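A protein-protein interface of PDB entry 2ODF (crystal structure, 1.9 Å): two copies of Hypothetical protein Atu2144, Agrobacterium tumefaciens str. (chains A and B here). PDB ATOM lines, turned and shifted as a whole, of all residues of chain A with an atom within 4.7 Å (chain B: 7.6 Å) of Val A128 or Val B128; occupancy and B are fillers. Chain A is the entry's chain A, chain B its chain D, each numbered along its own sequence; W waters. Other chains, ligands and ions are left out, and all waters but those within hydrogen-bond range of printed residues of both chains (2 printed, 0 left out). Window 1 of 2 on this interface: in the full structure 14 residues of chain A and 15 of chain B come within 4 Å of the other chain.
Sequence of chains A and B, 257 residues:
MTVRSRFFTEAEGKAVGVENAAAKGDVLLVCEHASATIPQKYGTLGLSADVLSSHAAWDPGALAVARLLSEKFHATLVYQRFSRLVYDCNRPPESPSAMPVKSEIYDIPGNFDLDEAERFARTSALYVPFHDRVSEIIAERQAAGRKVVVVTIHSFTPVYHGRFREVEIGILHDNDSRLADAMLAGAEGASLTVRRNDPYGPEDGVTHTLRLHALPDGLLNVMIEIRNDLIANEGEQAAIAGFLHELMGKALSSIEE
The side-chain carboxylate (OD1) of Asp A132 is in hydrogen-bond range of the side-chain hydroxyl (OG) of Ser B124, at 2.8 Å. The side-chain carboxylate (OD1) of Asp B132 lies within hydrogen-bond range of the side-chain hydroxyl (OG) of Ser A124, 2.6 Å away.
A ring nitrogen (NE2) of His B131 sits at hydrogen-bond distance from the backbone carbonyl oxygen (O) of Cys B89 (2.7 Å). The backbone carbonyl oxygen (O) of His B131 is in hydrogen-bond range of the side-chain hydroxyl (OG) of Ser B135. O of Thr A123 lies within hydrogen-bond range of N of Val A128 (3.0 Å). The backbone carbonyl oxygen (O) of Thr B123 sits at hydrogen-bond distance from the backbone NH (N) of Val B128, at 3.0 Å.
Among the printed residues, merely in contact across the chains: Phe A120 with His B131 (3.4 Å), Asp A132 with Phe B120 (3.4 Å), Phe A120 with Asp B132 (3.4 Å), His A131 with Phe B120 (3.5 Å), Tyr A127 with Phe B120 (3.6 Å), Val A128 with Ser B124 (3.6 Å), Phe A120 with Tyr B127 (3.7 Å), Ser A124 with Val B128 (3.9 Å) and Val A128 with Val B128 (3.9 Å).
Of the printed residues of chain B, Phe A120 touches Tyr B127, His B131 and Asp B132. Printed residues of chain B within 4 Å of Ser A124: Val B128 (3.9 Å) and Asp B132 (2.6 Å). Printed residues of chain B within 4 Å of Tyr A127: Phe B120. Val B128 touches just these residues of chain A: Ser A124 and Val A128. Of the printed residues of chain A, His B131 touches Phe A120. The nearest printed residue of chain B that does not touch Ser A124 is His B131 (6.7 Å).
Of the 20 printed residues of chain B, 6 touch a printed residue of chain A. Among the printed residues, 11 pairs touch across the chains.
Phe A120 touches Tyr B127, and with the chains exchanged Tyr A127 touches Phe B120. Phe A120 touches His B131, and with the chains exchanged His A131 touches Phe B120. Phe A120 touches Asp B132, and with the chains exchanged Asp A132 touches Phe B120. Ser A124 touches Val B128, and with the chains exchanged Val A128 touches Ser B124.
Water W2 lies within hydrogen-bond range of the backbone carbonyl oxygen (O) of Ser A124 and the side-chain carboxylate (OD2) of Asp B132. Water W1 bridges the backbone carbonyl oxygen (O) of Ser B124 (2.7 Å) and the side-chain carboxylate (OD2) of Asp A132 (3.0 Å).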
ATOM      1  N   PHE A 120      19.032 -19.030  21.267  1.00  0.00           N
ATOM      2  CA  PHE A 120      20.137 -19.953  21.181  1.00  0.00           C
ATOM      3  C   PHE A 120      21.109 -19.686  22.354  1.00  0.00           C
ATOM      4  O   PHE A 120      21.537 -20.613  22.990  1.00  0.00           O
ATOM      5  CB  PHE A 120      20.876 -19.906  19.835  1.00  0.00           C
ATOM      6  CG  PHE A 120      22.017 -20.836  19.803  1.00  0.00           C
ATOM      7  CD1 PHE A 120      21.811 -22.187  19.621  1.00  0.00           C
ATOM      8  CD2 PHE A 120      23.272 -20.409  20.150  1.00  0.00           C
ATOM      9  CE1 PHE A 120      22.863 -23.061  19.663  1.00  0.00           C
ATOM     10  CE2 PHE A 120      24.309 -21.277  20.210  1.00  0.00           C
ATOM     11  CZ  PHE A 120      24.101 -22.611  19.975  1.00  0.00           C
ATOM     12  N   THR A 123      19.701 -21.068  25.610  1.00  0.00           N
ATOM     13  CA  THR A 123      19.629 -22.515  25.521  1.00  0.00           C
ATOM     14  C   THR A 123      21.007 -23.173  25.675  1.00  0.00           C
ATOM     15  O   THR A 123      21.165 -24.182  26.375  1.00  0.00           O
ATOM     16  CB  THR A 123      18.970 -22.949  24.176  1.00  0.00           C
ATOM     17  OG1 THR A 123      17.651 -22.378  24.048  1.00  0.00           O
ATOM     18  CG2 THR A 123      18.881 -24.430  24.087  1.00  0.00           C
ATOM     19  N   SER A 124      22.009 -22.571  25.050  1.00  0.00           N
ATOM     20  CA  SER A 124      23.371 -23.092  25.043  1.00  0.00           C
ATOM     21  C   SER A 124      24.103 -22.934  26.358  1.00  0.00           C
ATOM     22  O   SER A 124      24.931 -23.764  26.689  1.00  0.00           O
ATOM     23  CB  SER A 124      24.216 -22.370  23.986  1.00  0.00           C
ATOM     24  OG  SER A 124      25.538 -22.856  24.023  1.00  0.00           O
ATOM     25  N   LEU A 126      22.669 -22.029  29.568  1.00  0.00           N
ATOM     26  CA  LEU A 126      21.961 -22.413  30.779  1.00  0.00           C
ATOM     27  C   LEU A 126      21.346 -23.788  30.720  1.00  0.00           C
ATOM     28  O   LEU A 126      21.569 -24.555  31.624  1.00  0.00           O
ATOM     29  CB  LEU A 126      20.883 -21.400  31.134  1.00  0.00           C
ATOM     30  CG  LEU A 126      21.406 -20.010  31.540  1.00  0.00           C
ATOM     31  CD1 LEU A 126      20.214 -19.067  31.664  1.00  0.00           C
ATOM     32  CD2 LEU A 126      22.292 -20.025  32.835  1.00  0.00           C
ATOM     33  N   TYR A 127      20.594 -24.106  29.658  1.00  0.00           N
ATOM     34  CA  TYR A 127      19.759 -25.300  29.640  1.00  0.00           C
ATOM     35  C   TYR A 127      20.559 -26.549  29.321  1.00  0.00           C
ATOM     36  O   TYR A 127      20.497 -27.544  30.066  1.00  0.00           O
ATOM     37  CB  TYR A 127      18.600 -25.087  28.642  1.00  0.00           C
ATOM     38  CG  TYR A 127      17.736 -26.281  28.344  1.00  0.00           C
ATOM     39  CD1 TYR A 127      16.798 -26.756  29.259  1.00  0.00           C
ATOM     40  CD2 TYR A 127      17.817 -26.914  27.101  1.00  0.00           C
ATOM     41  CE1 TYR A 127      15.967 -27.849  28.931  1.00  0.00           C
ATOM     42  CE2 TYR A 127      16.996 -27.960  26.779  1.00  0.00           C
ATOM     43  CZ  TYR A 127      16.090 -28.439  27.677  1.00  0.00           C
ATOM     44  OH  TYR A 127      15.321 -29.519  27.290  1.00  0.00           O
ATOM     45  N   VAL A 128      21.354 -26.493  28.254  1.00  0.00           N
ATOM     46  CA  VAL A 128      22.091 -27.679  27.827  1.00  0.00           C
ATOM     47  C   VAL A 128      23.179 -28.060  28.854  1.00  0.00           C
ATOM     48  O   VAL A 128      23.300 -29.233  29.185  1.00  0.00           O
ATOM     49  CB  VAL A 128      22.555 -27.612  26.323  1.00  0.00           C
ATOM     50  CG1 VAL A 128      23.473 -28.810  25.979  1.00  0.00           C
ATOM     51  CG2 VAL A 128      21.313 -27.613  25.372  1.00  0.00           C
ATOM     52  N   PRO A 129      23.986 -27.104  29.356  1.00  0.00           N
ATOM     53  CA  PRO A 129      24.973 -27.459  30.376  1.00  0.00           C
ATOM     54  C   PRO A 129      24.360 -28.105  31.617  1.00  0.00           C
ATOM     55  O   PRO A 129      24.887 -29.114  32.084  1.00  0.00           O
ATOM     56  CB  PRO A 129      25.666 -26.101  30.712  1.00  0.00           C
ATOM     57  CG  PRO A 129      25.511 -25.321  29.457  1.00  0.00           C
ATOM     58  CD  PRO A 129      24.149 -25.693  28.935  1.00  0.00           C
ATOM     59  N   PHE A 130      23.221 -27.600  32.077  1.00  0.00           N
ATOM     60  CA  PHE A 130      22.551 -28.123  33.241  1.00  0.00           C
ATOM     61  C   PHE A 130      22.160 -29.602  33.041  1.00  0.00           C
ATOM     62  O   PHE A 130      22.569 -30.468  33.823  1.00  0.00           O
ATOM     63  CB  PHE A 130      21.346 -27.246  33.617  1.00  0.00           C
ATOM     64  CG  PHE A 130      20.605 -27.730  34.824  1.00  0.00           C
ATOM     65  CD1 PHE A 130      21.120 -27.519  36.101  1.00  0.00           C
ATOM     66  CD2 PHE A 130      19.404 -28.416  34.690  1.00  0.00           C
ATOM     67  CE1 PHE A 130      20.440 -28.013  37.211  1.00  0.00           C
ATOM     68  CE2 PHE A 130      18.739 -28.913  35.796  1.00  0.00           C
ATOM     69  CZ  PHE A 130      19.260 -28.715  37.048  1.00  0.00           C
ATOM     70  N   HIS A 131      21.413 -29.879  31.999  1.00  0.00           N
ATOM     71  CA  HIS A 131      20.985 -31.201  31.718  1.00  0.00           C
ATOM     72  C   HIS A 131      22.106 -32.139  31.341  1.00  0.00           C
ATOM     73  O   HIS A 131      22.052 -33.273  31.650  1.00  0.00           O
ATOM     74  CB  HIS A 131      19.808 -31.202  30.780  1.00  0.00           C
ATOM     75  CG  HIS A 131      18.578 -30.611  31.384  1.00  0.00           C
ATOM     76  ND1 HIS A 131      17.869 -31.235  32.368  1.00  0.00           N
ATOM     77  CD2 HIS A 131      17.988 -29.417  31.196  1.00  0.00           C
ATOM     78  CE1 HIS A 131      16.879 -30.460  32.745  1.00  0.00           C
ATOM     79  NE2 HIS A 131      16.924 -29.359  32.038  1.00  0.00           N
ATOM     80  N   ASP A 132      23.119 -31.636  30.673  1.00  0.00           N
ATOM     81  CA  ASP A 132      24.250 -32.443  30.299  1.00  0.00           C
ATOM     82  C   ASP A 132      24.982 -32.945  31.569  1.00  0.00           C
ATOM     83  O   ASP A 132      25.467 -34.005  31.608  1.00  0.00           O
ATOM     84  CB  ASP A 132      25.202 -31.681  29.384  1.00  0.00           C
ATOM     85  CG  ASP A 132      24.789 -31.704  27.902  1.00  0.00           C
ATOM     86  OD1 ASP A 132      23.809 -32.325  27.533  1.00  0.00           O
ATOM     87  OD2 ASP A 132      25.483 -31.105  27.129  1.00  0.00           O
ATOM     88  N   VAL B  16      30.751 -32.149  14.733  1.00  0.00           N
ATOM     89  CA  VAL B  16      31.250 -30.952  14.070  1.00  0.00           C
ATOM     90  C   VAL B  16      32.587 -31.213  13.356  1.00  0.00           C
ATOM     91  O   VAL B  16      33.546 -31.716  13.956  1.00  0.00           O
ATOM     92  CB  VAL B  16      31.440 -29.796  15.060  1.00  0.00           C
ATOM     93  CG1 VAL B  16      31.771 -28.469  14.296  1.00  0.00           C
ATOM     94  CG2 VAL B  16      30.190 -29.593  15.910  1.00  0.00           C
ATOM     95  N   GLN B  80      28.737 -29.705   9.401  1.00  0.00           N
ATOM     96  CA  GLN B  80      28.035 -30.692  10.190  1.00  0.00           C
ATOM     97  C   GLN B  80      28.248 -32.040   9.494  1.00  0.00           C
ATOM     98  O   GLN B  80      28.112 -32.134   8.278  1.00  0.00           O
ATOM     99  CB  GLN B  80      26.572 -30.267  10.283  1.00  0.00           C
ATOM    100  CG  GLN B  80      25.598 -31.243  10.852  1.00  0.00           C
ATOM    101  CD  GLN B  80      25.924 -31.735  12.255  1.00  0.00           C
ATOM    102  OE1 GLN B  80      25.815 -31.004  13.244  1.00  0.00           O
ATOM    103  NE2 GLN B  80      26.256 -32.998  12.347  1.00  0.00           N
ATOM    104  N   TYR B  87      18.859 -33.916  12.851  1.00  0.00           N
ATOM    105  CA  TYR B  87      18.606 -32.551  13.277  1.00  0.00           C
ATOM    106  C   TYR B  87      19.003 -31.641  12.120  1.00  0.00           C
ATOM    107  O   TYR B  87      20.147 -31.684  11.652  1.00  0.00           O
ATOM    108  CB  TYR B  87      19.343 -32.164  14.579  1.00  0.00           C
ATOM    109  CG  TYR B  87      18.786 -30.871  15.146  1.00  0.00           C
ATOM    110  CD1 TYR B  87      19.043 -29.652  14.503  1.00  0.00           C
ATOM    111  CD2 TYR B  87      17.987 -30.852  16.304  1.00  0.00           C
ATOM    112  CE1 TYR B  87      18.509 -28.443  14.984  1.00  0.00           C
ATOM    113  CE2 TYR B  87      17.447 -29.630  16.793  1.00  0.00           C
ATOM    114  CZ  TYR B  87      17.700 -28.442  16.107  1.00  0.00           C
ATOM    115  OH  TYR B  87      17.148 -27.247  16.534  1.00  0.00           O
ATOM    116  N   CYS B  89      20.367 -28.539  11.352  1.00  0.00           N
ATOM    117  CA  CYS B  89      21.069 -27.493  12.117  1.00  0.00           C
ATOM    118  C   CYS B  89      20.777 -26.073  11.661  1.00  0.00           C
ATOM    119  O   CYS B  89      21.142 -25.131  12.374  1.00  0.00           O
ATOM    120  CB  CYS B  89      22.592 -27.716  12.113  1.00  0.00           C
ATOM    121  SG  CYS B  89      23.088 -29.106  13.164  1.00  0.00           S
ATOM    122  N   PRO B  93      15.052 -25.458  17.575  1.00  0.00           N
ATOM    123  CA  PRO B  93      14.285 -26.599  18.041  1.00  0.00           C
ATOM    124  C   PRO B  93      12.762 -26.395  18.022  1.00  0.00           C
ATOM    125  O   PRO B  93      12.014 -27.365  17.873  1.00  0.00           O
ATOM    126  CB  PRO B  93      14.803 -26.839  19.474  1.00  0.00           C
ATOM    127  CG  PRO B  93      15.883 -25.897  19.710  1.00  0.00           C
ATOM    128  CD  PRO B  93      16.025 -24.971  18.560  1.00  0.00           C
ATOM    129  N   PHE B 120      16.020 -33.806  23.278  1.00  0.00           N
ATOM    130  CA  PHE B 120      17.149 -33.192  23.974  1.00  0.00           C
ATOM    131  C   PHE B 120      18.436 -33.805  23.453  1.00  0.00           C
ATOM    132  O   PHE B 120      19.431 -33.105  23.200  1.00  0.00           O
ATOM    133  CB  PHE B 120      17.085 -33.388  25.475  1.00  0.00           C
ATOM    134  CG  PHE B 120      18.240 -32.779  26.173  1.00  0.00           C
ATOM    135  CD1 PHE B 120      18.224 -31.445  26.496  1.00  0.00           C
ATOM    136  CD2 PHE B 120      19.383 -33.509  26.430  1.00  0.00           C
ATOM    137  CE1 PHE B 120      19.289 -30.851  27.130  1.00  0.00           C
ATOM    138  CE2 PHE B 120      20.495 -32.908  27.039  1.00  0.00           C
ATOM    139  CZ  PHE B 120      20.430 -31.573  27.385  1.00  0.00           C
ATOM    140  N   ARG B 122      19.198 -35.176  20.506  1.00  0.00           N
ATOM    141  CA  ARG B 122      19.528 -34.618  19.209  1.00  0.00           C
ATOM    142  C   ARG B 122      19.943 -33.158  19.302  1.00  0.00           C
ATOM    143  O   ARG B 122      20.898 -32.732  18.645  1.00  0.00           O
ATOM    144  CB  ARG B 122      18.350 -34.771  18.276  1.00  0.00           C
ATOM    145  CG  ARG B 122      17.997 -36.233  17.984  1.00  0.00           C
ATOM    146  CD  ARG B 122      17.006 -36.255  16.884  1.00  0.00           C
ATOM    147  NE  ARG B 122      16.340 -37.542  16.772  1.00  0.00           N
ATOM    148  CZ  ARG B 122      15.662 -37.947  15.693  1.00  0.00           C
ATOM    149  NH1 ARG B 122      15.551 -37.178  14.620  1.00  0.00           N
ATOM    150  NH2 ARG B 122      15.064 -39.136  15.715  1.00  0.00           N
ATOM    151  N   THR B 123      19.283 -32.400  20.159  1.00  0.00           N
ATOM    152  CA  THR B 123      19.610 -30.979  20.313  1.00  0.00           C
ATOM    153  C   THR B 123      21.008 -30.803  20.911  1.00  0.00           C
ATOM    154  O   THR B 123      21.821 -30.089  20.369  1.00  0.00           O
ATOM    155  CB  THR B 123      18.526 -30.284  21.162  1.00  0.00           C
ATOM    156  OG1 THR B 123      17.267 -30.513  20.522  1.00  0.00           O
ATOM    157  CG2 THR B 123      18.740 -28.797  21.259  1.00  0.00           C
ATOM    158  N   SER B 124      21.291 -31.525  21.993  1.00  0.00           N
ATOM    159  CA  SER B 124      22.574 -31.501  22.673  1.00  0.00           C
ATOM    160  C   SER B 124      23.745 -32.091  21.859  1.00  0.00           C
ATOM    161  O   SER B 124      24.870 -31.581  21.961  1.00  0.00           O
ATOM    162  CB  SER B 124      22.450 -32.247  24.005  1.00  0.00           C
ATOM    163  OG  SER B 124      23.639 -32.188  24.762  1.00  0.00           O
ATOM    164  N   ALA B 125      23.490 -33.131  21.055  1.00  0.00           N
ATOM    165  CA  ALA B 125      24.559 -33.820  20.283  1.00  0.00           C
ATOM    166  C   ALA B 125      24.934 -33.162  18.970  1.00  0.00           C
ATOM    167  O   ALA B 125      26.145 -33.144  18.561  1.00  0.00           O
ATOM    168  CB  ALA B 125      24.196 -35.289  20.033  1.00  0.00           C
ATOM    169  N   LEU B 126      23.928 -32.656  18.269  1.00  0.00           N
ATOM    170  CA  LEU B 126      24.130 -32.131  16.916  1.00  0.00           C
ATOM    171  C   LEU B 126      24.061 -30.617  16.800  1.00  0.00           C
ATOM    172  O   LEU B 126      24.992 -29.985  16.313  1.00  0.00           O
ATOM    173  CB  LEU B 126      23.117 -32.748  15.962  1.00  0.00           C
ATOM    174  CG  LEU B 126      23.278 -34.256  15.745  1.00  0.00           C
ATOM    175  CD1 LEU B 126      22.135 -34.763  14.884  1.00  0.00           C
ATOM    176  CD2 LEU B 126      24.596 -34.529  15.071  1.00  0.00           C
ATOM    177  N   TYR B 127      22.971 -30.043  17.282  1.00  0.00           N
ATOM    178  CA  TYR B 127      22.670 -28.639  17.081  1.00  0.00           C
ATOM    179  C   TYR B 127      23.536 -27.684  17.909  1.00  0.00           C
ATOM    180  O   TYR B 127      24.217 -26.776  17.383  1.00  0.00           O
ATOM    181  CB  TYR B 127      21.190 -28.449  17.405  1.00  0.00           C
ATOM    182  CG  TYR B 127      20.668 -27.034  17.334  1.00  0.00           C
ATOM    183  CD1 TYR B 127      20.558 -26.368  16.111  1.00  0.00           C
ATOM    184  CD2 TYR B 127      20.258 -26.364  18.497  1.00  0.00           C
ATOM    185  CE1 TYR B 127      20.083 -25.089  16.056  1.00  0.00           C
ATOM    186  CE2 TYR B 127      19.771 -25.072  18.437  1.00  0.00           C
ATOM    187  CZ  TYR B 127      19.673 -24.448  17.206  1.00  0.00           C
ATOM    188  OH  TYR B 127      19.188 -23.171  17.082  1.00  0.00           O
ATOM    189  N   VAL B 128      23.521 -27.871  19.217  1.00  0.00           N
ATOM    190  CA  VAL B 128      24.232 -26.953  20.073  1.00  0.00           C
ATOM    191  C   VAL B 128      25.771 -26.998  19.850  1.00  0.00           C
ATOM    192  O   VAL B 128      26.388 -25.970  19.786  1.00  0.00           O
ATOM    193  CB  VAL B 128      23.793 -27.127  21.548  1.00  0.00           C
ATOM    194  CG1 VAL B 128      24.701 -26.310  22.487  1.00  0.00           C
ATOM    195  CG2 VAL B 128      22.308 -26.750  21.719  1.00  0.00           C
ATOM    196  N   PRO B 129      26.398 -28.183  19.729  1.00  0.00           N
ATOM    197  CA  PRO B 129      27.856 -28.193  19.443  1.00  0.00           C
ATOM    198  C   PRO B 129      28.251 -27.481  18.142  1.00  0.00           C
ATOM    199  O   PRO B 129      29.321 -26.833  18.070  1.00  0.00           O
ATOM    200  CB  PRO B 129      28.171 -29.689  19.365  1.00  0.00           C
ATOM    201  CG  PRO B 129      27.155 -30.309  20.265  1.00  0.00           C
ATOM    202  CD  PRO B 129      25.900 -29.536  20.003  1.00  0.00           C
ATOM    203  N   PHE B 130      27.416 -27.627  17.123  1.00  0.00           N
ATOM    204  CA  PHE B 130      27.654 -27.020  15.817  1.00  0.00           C
ATOM    205  C   PHE B 130      27.711 -25.495  15.894  1.00  0.00           C
ATOM    206  O   PHE B 130      28.697 -24.872  15.496  1.00  0.00           O
ATOM    207  CB  PHE B 130      26.628 -27.510  14.791  1.00  0.00           C
ATOM    208  CG  PHE B 130      26.798 -26.884  13.413  1.00  0.00           C
ATOM    209  CD1 PHE B 130      27.792 -27.323  12.545  1.00  0.00           C
ATOM    210  CD2 PHE B 130      25.986 -25.873  13.000  1.00  0.00           C
ATOM    211  CE1 PHE B 130      27.965 -26.753  11.311  1.00  0.00           C
ATOM    212  CE2 PHE B 130      26.143 -25.302  11.723  1.00  0.00           C
ATOM    213  CZ  PHE B 130      27.156 -25.752  10.897  1.00  0.00           C
ATOM    214  N   HIS B 131      26.661 -24.901  16.435  1.00  0.00           N
ATOM    215  CA  HIS B 131      26.590 -23.474  16.573  1.00  0.00           C
ATOM    216  C   HIS B 131      27.521 -22.921  17.641  1.00  0.00           C
ATOM    217  O   HIS B 131      28.045 -21.821  17.486  1.00  0.00           O
ATOM    218  CB  HIS B 131      25.140 -23.055  16.809  1.00  0.00           C
ATOM    219  CG  HIS B 131      24.287 -23.216  15.594  1.00  0.00           C
ATOM    220  ND1 HIS B 131      24.511 -22.490  14.439  1.00  0.00           N
ATOM    221  CD2 HIS B 131      23.301 -24.094  15.301  1.00  0.00           C
ATOM    222  CE1 HIS B 131      23.668 -22.886  13.505  1.00  0.00           C
ATOM    223  NE2 HIS B 131      22.919 -23.855  13.999  1.00  0.00           N
ATOM    224  N   ASP B 132      27.715 -23.658  18.739  1.00  0.00           N
ATOM    225  CA  ASP B 132      28.734 -23.256  19.726  1.00  0.00           C
ATOM    226  C   ASP B 132      30.115 -23.106  19.096  1.00  0.00           C
ATOM    227  O   ASP B 132      30.858 -22.175  19.412  1.00  0.00           O
ATOM    228  CB  ASP B 132      28.823 -24.263  20.867  1.00  0.00           C
ATOM    229  CG  ASP B 132      27.769 -24.035  21.942  1.00  0.00           C
ATOM    230  OD1 ASP B 132      26.964 -23.068  21.832  1.00  0.00           O
ATOM    231  OD2 ASP B 132      27.761 -24.839  22.920  1.00  0.00           O
ATOM    232  N   ARG B 133      30.463 -24.014  18.236  1.00  0.00           N
ATOM    233  CA  ARG B 133      31.738 -23.948  17.558  1.00  0.00           C
ATOM    234  C   ARG B 133      31.869 -22.724  16.643  1.00  0.00           C
ATOM    235  O   ARG B 133      32.834 -22.036  16.711  1.00  0.00           O
ATOM    236  CB  ARG B 133      32.068 -25.208  16.814  1.00  0.00           C
ATOM    237  CG  ARG B 133      33.458 -25.243  16.314  1.00  0.00           C
ATOM    238  CD  ARG B 133      34.437 -25.751  17.379  1.00  0.00           C
ATOM    239  NE  ARG B 133      35.779 -25.471  16.964  1.00  0.00           N
ATOM    240  CZ  ARG B 133      36.610 -26.382  16.513  1.00  0.00           C
ATOM    241  NH1 ARG B 133      36.242 -27.650  16.472  1.00  0.00           N
ATOM    242  NH2 ARG B 133      37.807 -26.016  16.130  1.00  0.00           N
ATOM    243  N   VAL B 134      30.838 -22.473  15.851  1.00  0.00           N
ATOM    244  CA  VAL B 134      30.797 -21.298  14.983  1.00  0.00           C
ATOM    245  C   VAL B 134      30.919 -20.026  15.830  1.00  0.00           C
ATOM    246  O   VAL B 134      31.741 -19.150  15.524  1.00  0.00           O
ATOM    247  CB  VAL B 134      29.515 -21.265  14.117  1.00  0.00           C
ATOM    248  CG1 VAL B 134      29.449 -19.996  13.263  1.00  0.00           C
ATOM    249  CG2 VAL B 134      29.443 -22.507  13.207  1.00  0.00           C
ATOM    250  N   SER B 135      30.128 -19.947  16.910  1.00  0.00           N
ATOM    251  CA  SER B 135      30.159 -18.801  17.824  1.00  0.00           C
ATOM    252  C   SER B 135      31.536 -18.584  18.486  1.00  0.00           C
ATOM    253  O   SER B 135      31.979 -17.436  18.655  1.00  0.00           O
ATOM    254  CB  SER B 135      29.109 -18.970  18.930  1.00  0.00           C
ATOM    255  OG  SER B 135      27.808 -18.706  18.454  1.00  0.00           O
HETATM  256  O   HOH W   1      25.867 -30.436  24.232  1.00  0.00           O
HETATM  257  O   HOH W   2      26.487 -25.347  25.449  1.00  0.00           O
